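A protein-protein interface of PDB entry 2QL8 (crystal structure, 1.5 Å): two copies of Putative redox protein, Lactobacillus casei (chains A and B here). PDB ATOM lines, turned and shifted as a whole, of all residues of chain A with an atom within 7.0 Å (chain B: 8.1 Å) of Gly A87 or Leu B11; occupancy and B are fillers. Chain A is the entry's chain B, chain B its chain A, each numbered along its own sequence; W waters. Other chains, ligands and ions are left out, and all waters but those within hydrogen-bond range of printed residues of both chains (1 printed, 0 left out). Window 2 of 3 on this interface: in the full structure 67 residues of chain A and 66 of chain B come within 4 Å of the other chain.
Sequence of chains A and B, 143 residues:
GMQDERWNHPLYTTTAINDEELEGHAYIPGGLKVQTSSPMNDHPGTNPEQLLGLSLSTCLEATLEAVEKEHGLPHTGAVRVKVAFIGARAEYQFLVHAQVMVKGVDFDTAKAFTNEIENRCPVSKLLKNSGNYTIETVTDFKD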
ATOM      1  N   PRO A  39       9.113   6.114 -25.638  1.00  0.00           N
ATOM      2  CA  PRO A  39       7.728   6.581 -25.618  1.00  0.00           C
ATOM      3  C   PRO A  39       6.992   6.489 -26.959  1.00  0.00           C
ATOM      4  O   PRO A  39       5.766   6.638 -27.019  1.00  0.00           O
ATOM      5  CB  PRO A  39       7.869   8.040 -25.218  1.00  0.00           C
ATOM      6  CG  PRO A  39       9.210   8.439 -25.674  1.00  0.00           C
ATOM      7  CD  PRO A  39      10.081   7.223 -25.478  1.00  0.00           C
ATOM      8  N   MET A  40       7.735   6.215 -28.016  1.00  0.00           N
ATOM      9  CA  MET A  40       7.171   6.184 -29.367  1.00  0.00           C
ATOM     10  C   MET A  40       6.601   4.825 -29.744  1.00  0.00           C
ATOM     11  O   MET A  40       6.139   4.651 -30.867  1.00  0.00           O
ATOM     12  CB  MET A  40       8.214   6.675 -30.373  1.00  0.00           C
ATOM     13  CG  MET A  40       8.756   8.052 -30.079  1.00  0.00           C
ATOM     14  SD  MET A  40       7.402   9.409 -29.868  1.00  0.00           S
ATOM     15  CE  MET A  40       6.817   9.516 -31.710  1.00  0.00           C
ATOM     16  N   ALA A  84       6.106  17.243 -22.631  1.00  0.00           N
ATOM     17  CA  ALA A  84       6.031  17.011 -24.085  1.00  0.00           C
ATOM     18  C   ALA A  84       7.424  16.747 -24.644  1.00  0.00           C
ATOM     19  O   ALA A  84       8.376  17.394 -24.256  1.00  0.00           O
ATOM     20  CB  ALA A  84       5.388  18.204 -24.791  1.00  0.00           C
ATOM     21  N   PHE A  85       7.484  15.840 -25.620  1.00  0.00           N
ATOM     22  CA  PHE A  85       8.645  15.517 -26.398  1.00  0.00           C
ATOM     23  C   PHE A  85       8.393  16.096 -27.783  1.00  0.00           C
ATOM     24  O   PHE A  85       7.368  15.797 -28.402  1.00  0.00           O
ATOM     25  CB  PHE A  85       8.771  14.021 -26.410  1.00  0.00           C
ATOM     26  CG  PHE A  85       9.883  13.444 -27.260  1.00  0.00           C
ATOM     27  CD1 PHE A  85      11.195  13.941 -27.230  1.00  0.00           C
ATOM     28  CD2 PHE A  85       9.619  12.333 -28.068  1.00  0.00           C
ATOM     29  CE1 PHE A  85      12.175  13.344 -27.960  1.00  0.00           C
ATOM     30  CE2 PHE A  85      10.626  11.767 -28.815  1.00  0.00           C
ATOM     31  CZ  PHE A  85      11.885  12.271 -28.755  1.00  0.00           C
ATOM     32  N   ILE A  86       9.328  16.956 -28.216  1.00  0.00           N
ATOM     33  CA  ILE A  86       9.224  17.621 -29.506  1.00  0.00           C
ATOM     34  C   ILE A  86      10.571  17.543 -30.261  1.00  0.00           C
ATOM     35  O   ILE A  86      11.631  17.295 -29.668  1.00  0.00           O
ATOM     36  CB  ILE A  86       8.805  19.142 -29.374  1.00  0.00           C
ATOM     37  CG1 ILE A  86       9.928  19.991 -28.741  1.00  0.00           C
ATOM     38  CG2 ILE A  86       7.466  19.271 -28.607  1.00  0.00           C
ATOM     39  CD1 ILE A  86       9.624  21.471 -28.664  1.00  0.00           C
ATOM     40  N   GLY A  87      10.498  17.730 -31.587  1.00  0.00           N
ATOM     41  CA  GLY A  87      11.687  17.898 -32.372  1.00  0.00           C
ATOM     42  C   GLY A  87      11.894  16.853 -33.440  1.00  0.00           C
ATOM     43  O   GLY A  87      10.964  16.324 -33.995  1.00  0.00           O
ATOM     44  N   ALA A  88      13.161  16.609 -33.708  1.00  0.00           N
ATOM     45  CA  ALA A  88      13.605  15.682 -34.738  1.00  0.00           C
ATOM     46  C   ALA A  88      15.018  15.215 -34.380  1.00  0.00           C
ATOM     47  O   ALA A  88      15.603  15.724 -33.445  1.00  0.00           O
ATOM     48  CB  ALA A  88      13.534  16.323 -36.152  1.00  0.00           C
ATOM     49  N   ARG A  89      15.546  14.250 -35.125  1.00  0.00           N
ATOM     50  CA  ARG A  89      16.884  13.709 -34.873  1.00  0.00           C
ATOM     51  C   ARG A  89      17.905  14.782 -34.550  1.00  0.00           C
ATOM     52  O   ARG A  89      18.073  15.745 -35.311  1.00  0.00           O
ATOM     53  CB  ARG A  89      17.382  12.944 -36.101  1.00  0.00           C
ATOM     54  CG  ARG A  89      18.649  12.115 -35.843  1.00  0.00           C
ATOM     55  CD  ARG A  89      19.418  11.787 -37.176  1.00  0.00           C
ATOM     56  NE  ARG A  89      19.989  13.020 -37.703  1.00  0.00           N
ATOM     57  CZ  ARG A  89      21.121  13.562 -37.273  1.00  0.00           C
ATOM     58  NH1 ARG A  89      21.872  12.944 -36.326  1.00  0.00           N
ATOM     59  NH2 ARG A  89      21.523  14.721 -37.794  1.00  0.00           N
ATOM     60  N   GLU A  91      17.811  17.065 -32.570  1.00  0.00           N
ATOM     61  CA  GLU A  91      17.130  18.350 -32.336  1.00  0.00           C
ATOM     62  C   GLU A  91      15.895  18.075 -31.466  1.00  0.00           C
ATOM     63  O   GLU A  91      14.823  18.613 -31.701  1.00  0.00           O
ATOM     64  CB  GLU A  91      16.686  18.990 -33.663  1.00  0.00           C
ATOM     65  CG  GLU A  91      17.825  19.442 -34.548  1.00  0.00           C
ATOM     66  CD  GLU A  91      18.604  20.624 -34.014  1.00  0.00           C
ATOM     67  OE1 GLU A  91      18.246  21.209 -32.954  1.00  0.00           O
ATOM     68  OE2 GLU A  91      19.601  21.002 -34.701  1.00  0.00           O
ATOM     69  N   TYR A  92      16.044  17.240 -30.446  1.00  0.00           N
ATOM     70  CA  TYR A  92      14.919  16.919 -29.554  1.00  0.00           C
ATOM     71  C   TYR A  92      14.953  17.760 -28.294  1.00  0.00           C
ATOM     72  O   TYR A  92      16.024  18.137 -27.786  1.00  0.00           O
ATOM     73  CB  TYR A  92      14.940  15.445 -29.167  1.00  0.00           C
ATOM     74  CG  TYR A  92      14.645  14.506 -30.300  1.00  0.00           C
ATOM     75  CD1 TYR A  92      13.409  14.530 -30.929  1.00  0.00           C
ATOM     76  CD2 TYR A  92      15.546  13.541 -30.691  1.00  0.00           C
ATOM     77  CE1 TYR A  92      13.100  13.664 -31.960  1.00  0.00           C
ATOM     78  CE2 TYR A  92      15.248  12.651 -31.705  1.00  0.00           C
ATOM     79  CZ  TYR A  92      14.010  12.693 -32.331  1.00  0.00           C
ATOM     80  OH  TYR A  92      13.674  11.836 -33.400  1.00  0.00           O
ATOM     81  N   GLN A  93      13.755  18.074 -27.816  1.00  0.00           N
ATOM     82  CA  GLN A  93      13.597  18.822 -26.560  1.00  0.00           C
ATOM     83  C   GLN A  93      12.416  18.286 -25.774  1.00  0.00           C
ATOM     84  O   GLN A  93      11.532  17.600 -26.308  1.00  0.00           O
ATOM     85  CB  GLN A  93      13.353  20.298 -26.798  1.00  0.00           C
ATOM     86  CG  GLN A  93      14.434  21.039 -27.575  1.00  0.00           C
ATOM     87  CD  GLN A  93      14.148  22.502 -27.666  1.00  0.00           C
ATOM     88  OE1 GLN A  93      14.214  23.206 -26.652  1.00  0.00           O
ATOM     89  NE2 GLN A  93      13.720  22.963 -28.870  1.00  0.00           N
ATOM     90  N   ARG B   6       5.112  25.837 -29.238  1.00  0.00           N
ATOM     91  CA  ARG B   6       5.837  24.574 -29.254  1.00  0.00           C
ATOM     92  C   ARG B   6       5.033  23.413 -28.644  1.00  0.00           C
ATOM     93  O   ARG B   6       5.387  22.259 -28.829  1.00  0.00           O
ATOM     94  CB  ARG B   6       7.200  24.702 -28.605  1.00  0.00           C
ATOM     95  CG  ARG B   6       8.112  25.683 -29.285  1.00  0.00           C
ATOM     96  CD  ARG B   6       9.457  25.805 -28.619  1.00  0.00           C
ATOM     97  NE  ARG B   6       9.266  26.292 -27.268  1.00  0.00           N
ATOM     98  CZ  ARG B   6      10.185  26.238 -26.311  1.00  0.00           C
ATOM     99  NH1 ARG B   6      11.383  25.754 -26.539  1.00  0.00           N
ATOM    100  NH2 ARG B   6       9.885  26.671 -25.109  1.00  0.00           N
ATOM    101  N   TRP B   7       3.967  23.718 -27.896  1.00  0.00           N
ATOM    102  CA  TRP B   7       3.054  22.694 -27.416  1.00  0.00           C
ATOM    103  C   TRP B   7       1.996  22.260 -28.416  1.00  0.00           C
ATOM    104  O   TRP B   7       1.207  21.361 -28.110  1.00  0.00           O
ATOM    105  CB  TRP B   7       2.342  23.220 -26.172  1.00  0.00           C
ATOM    106  CG  TRP B   7       3.179  23.170 -24.902  1.00  0.00           C
ATOM    107  CD1 TRP B   7       3.995  24.148 -24.432  1.00  0.00           C
ATOM    108  CD2 TRP B   7       3.302  22.071 -24.000  1.00  0.00           C
ATOM    109  NE1 TRP B   7       4.594  23.743 -23.263  1.00  0.00           N
ATOM    110  CE2 TRP B   7       4.176  22.477 -22.965  1.00  0.00           C
ATOM    111  CE3 TRP B   7       2.728  20.811 -23.936  1.00  0.00           C
ATOM    112  CZ2 TRP B   7       4.508  21.635 -21.881  1.00  0.00           C
ATOM    113  CZ3 TRP B   7       3.046  19.976 -22.863  1.00  0.00           C
ATOM    114  CH2 TRP B   7       3.947  20.396 -21.849  1.00  0.00           C
ATOM    115  N   ASN B   8       1.963  22.858 -29.617  1.00  0.00           N
ATOM    116  CA  ASN B   8       0.799  22.648 -30.491  1.00  0.00           C
ATOM    117  C   ASN B   8       0.655  21.240 -31.075  1.00  0.00           C
ATOM    118  O   ASN B   8      -0.495  20.792 -31.319  1.00  0.00           O
ATOM    119  CB  ASN B   8       0.812  23.680 -31.606  1.00  0.00           C
ATOM    120  CG  ASN B   8       0.238  25.010 -31.188  1.00  0.00           C
ATOM    121  OD1 ASN B   8      -0.060  25.260 -30.010  1.00  0.00           O
ATOM    122  ND2 ASN B   8       0.115  25.911 -32.163  1.00  0.00           N
ATOM    123  N   HIS B   9       1.763  20.540 -31.337  1.00  0.00           N
ATOM    124  CA  HIS B   9       1.672  19.183 -31.901  1.00  0.00           C
ATOM    125  C   HIS B   9       2.887  18.357 -31.563  1.00  0.00           C
ATOM    126  O   HIS B   9       3.742  18.100 -32.407  1.00  0.00           O
ATOM    127  CB  HIS B   9       1.445  19.267 -33.410  1.00  0.00           C
ATOM    128  CG  HIS B   9       1.232  17.961 -34.070  1.00  0.00           C
ATOM    129  ND1 HIS B   9       0.171  17.149 -33.762  1.00  0.00           N
ATOM    130  CD2 HIS B   9       1.909  17.349 -35.080  1.00  0.00           C
ATOM    131  CE1 HIS B   9       0.230  16.054 -34.515  1.00  0.00           C
ATOM    132  NE2 HIS B   9       1.271  16.155 -35.325  1.00  0.00           N
ATOM    133  N   PRO B  10       3.004  17.945 -30.289  1.00  0.00           N
ATOM    134  CA  PRO B  10       4.225  17.205 -29.910  1.00  0.00           C
ATOM    135  C   PRO B  10       4.317  15.796 -30.500  1.00  0.00           C
ATOM    136  O   PRO B  10       3.314  15.220 -30.980  1.00  0.00           O
ATOM    137  CB  PRO B  10       4.114  17.146 -28.362  1.00  0.00           C
ATOM    138  CG  PRO B  10       3.201  18.289 -28.026  1.00  0.00           C
ATOM    139  CD  PRO B  10       2.173  18.261 -29.126  1.00  0.00           C
ATOM    140  N   LEU B  11       5.515  15.225 -30.431  1.00  0.00           N
ATOM    141  CA  LEU B  11       5.705  13.816 -30.739  1.00  0.00           C
ATOM    142  C   LEU B  11       5.033  12.883 -29.728  1.00  0.00           C
ATOM    143  O   LEU B  11       4.556  11.779 -30.073  1.00  0.00           O
ATOM    144  CB  LEU B  11       7.198  13.490 -30.819  1.00  0.00           C
ATOM    145  CG  LEU B  11       8.023  14.328 -31.797  1.00  0.00           C
ATOM    146  CD1 LEU B  11       9.531  14.007 -31.611  1.00  0.00           C
ATOM    147  CD2 LEU B  11       7.556  14.144 -33.245  1.00  0.00           C
ATOM    148  N   TYR B  12       5.033  13.330 -28.461  1.00  0.00           N
ATOM    149  CA  TYR B  12       4.537  12.541 -27.352  1.00  0.00           C
ATOM    150  C   TYR B  12       4.299  13.474 -26.190  1.00  0.00           C
ATOM    151  O   TYR B  12       5.044  14.416 -26.005  1.00  0.00           O
ATOM    152  CB  TYR B  12       5.584  11.501 -26.953  1.00  0.00           C
ATOM    153  CG  TYR B  12       5.334  10.740 -25.656  1.00  0.00           C
ATOM    154  CD1 TYR B  12       4.457   9.671 -25.606  1.00  0.00           C
ATOM    155  CD2 TYR B  12       5.966  11.089 -24.485  1.00  0.00           C
ATOM    156  CE1 TYR B  12       4.226   8.949 -24.434  1.00  0.00           C
ATOM    157  CE2 TYR B  12       5.769  10.370 -23.307  1.00  0.00           C
ATOM    158  CZ  TYR B  12       4.899   9.303 -23.278  1.00  0.00           C
ATOM    159  OH  TYR B  12       4.701   8.586 -22.119  1.00  0.00           O
ATOM    160  N   THR B  13       3.256  13.207 -25.450  1.00  0.00           N
ATOM    161  CA  THR B  13       3.003  13.898 -24.189  1.00  0.00           C
ATOM    162  C   THR B  13       2.626  12.896 -23.115  1.00  0.00           C
ATOM    163  O   THR B  13       2.065  11.831 -23.399  1.00  0.00           O
ATOM    164  CB  THR B  13       1.847  14.937 -24.284  1.00  0.00           C
ATOM    165  OG1 THR B  13       0.597  14.265 -24.498  1.00  0.00           O
ATOM    166  CG2 THR B  13       2.097  15.968 -25.390  1.00  0.00           C
ATOM    167  N   LYS B 125      19.788  19.215 -21.830  1.00  0.00           N
ATOM    168  CA  LYS B 125      19.536  20.561 -22.303  1.00  0.00           C
ATOM    169  C   LYS B 125      18.713  21.381 -21.285  1.00  0.00           C
ATOM    170  O   LYS B 125      18.961  22.572 -21.098  1.00  0.00           O
ATOM    171  CB  LYS B 125      18.814  20.532 -23.648  1.00  0.00           C
ATOM    172  CG  LYS B 125      19.625  20.041 -24.794  1.00  0.00           C
ATOM    173  CD  LYS B 125      18.656  20.132 -26.055  1.00  0.00           C
ATOM    174  CE  LYS B 125      19.049  19.371 -27.143  1.00  0.00           C
ATOM    175  NZ  LYS B 125      18.177  19.670 -28.279  1.00  0.00           N
HETATM  176  O   HOH W   1      12.949  25.854 -29.034  1.00  0.00           O
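The backbone carbonyl oxygen (O) of Ile A86 is in hydrogen-bond range of the backbone NH (N) of Gln A93 (2.9 Å).
Among the printed residues, pairs that only touch across the chains: Pro A39 with Tyr B12, Ala A84 with Trp B7, Ala A84 with Pro B10, Ala A84 with Tyr B12, Phe A85 with Pro B10, Ile A86 with Arg B6, Ile A86 with Pro B10, Ile A86 with Leu B11, Gly A87 with Leu B11, Tyr A92 with Leu B11 and Gln A93 with Arg B6.
No position is printed for both chains. Of the 15 pairs that touch across the chains among the printed residues, none has its exchanged pair printed and touching as well.
Water W1 bridges NH1 of Arg B6 and NE2 of Gln A93.
Of the printed residues of chain B, Gly A87 touches Leu B11 (3.6 Å). Leu B11 touches just these residues of chain A: Met A40 (3.6 Å), Phe A85 (2.8 Å), Ile A86 (3.9 Å), Gly A87 (3.6 Å) and Tyr A92 (3.6 Å). No residue of chain B comes within 4 Å of Ala A88. Of the printed residues of chain B, Ile A86 touches Arg B6 (3.6 Å), Pro B10 (3.98 Å) and Leu B11 (3.9 Å). Printed residues of chain B within 4 Å of Gln A93: Arg B6. The nearest residue of chain B that does not touch Gly A87 is Pro B10 (6.5 Å). The nearest printed residue of chain B that does not touch Tyr A92 is Tyr B12 (8.8 Å).
O of Phe A85 sits at hydrogen-bond distance from N of Leu B11 (2.8 Å). The side-chain sulfur (SD) of Met A40 sits close to the backbone carbonyl oxygen (O) of Leu B11 (3.7 Å). The backbone carbonyl oxygen (O) of Tyr A92 sits at hydrogen-bond distance from the side-chain amino group (NZ) of Lys B125, at 2.7 Å. The backbone NH (N) of Phe A85 is in hydrogen-bond range of the backbone carbonyl oxygen (O) of Tyr B12 (2.9 Å).
Hydrophobic or aromatic side chains of chain B that line the printed part of chain A: Trp B7, Pro B10, Leu B11 and Tyr B12. Along chain B the printed residues that touch a printed residue of chain A span positions 6 to 125. Printed residues of chain A that touch a printed residue of chain B: Pro A39, Met A40, Ala A84, Phe A85, Ile A86, Gly A87, Tyr A92 and Gln A93. Among the printed residues, no Asp or Glu carboxylate lies within 4 Å of a Lys or Arg side-chain nitrogen of the other chain.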
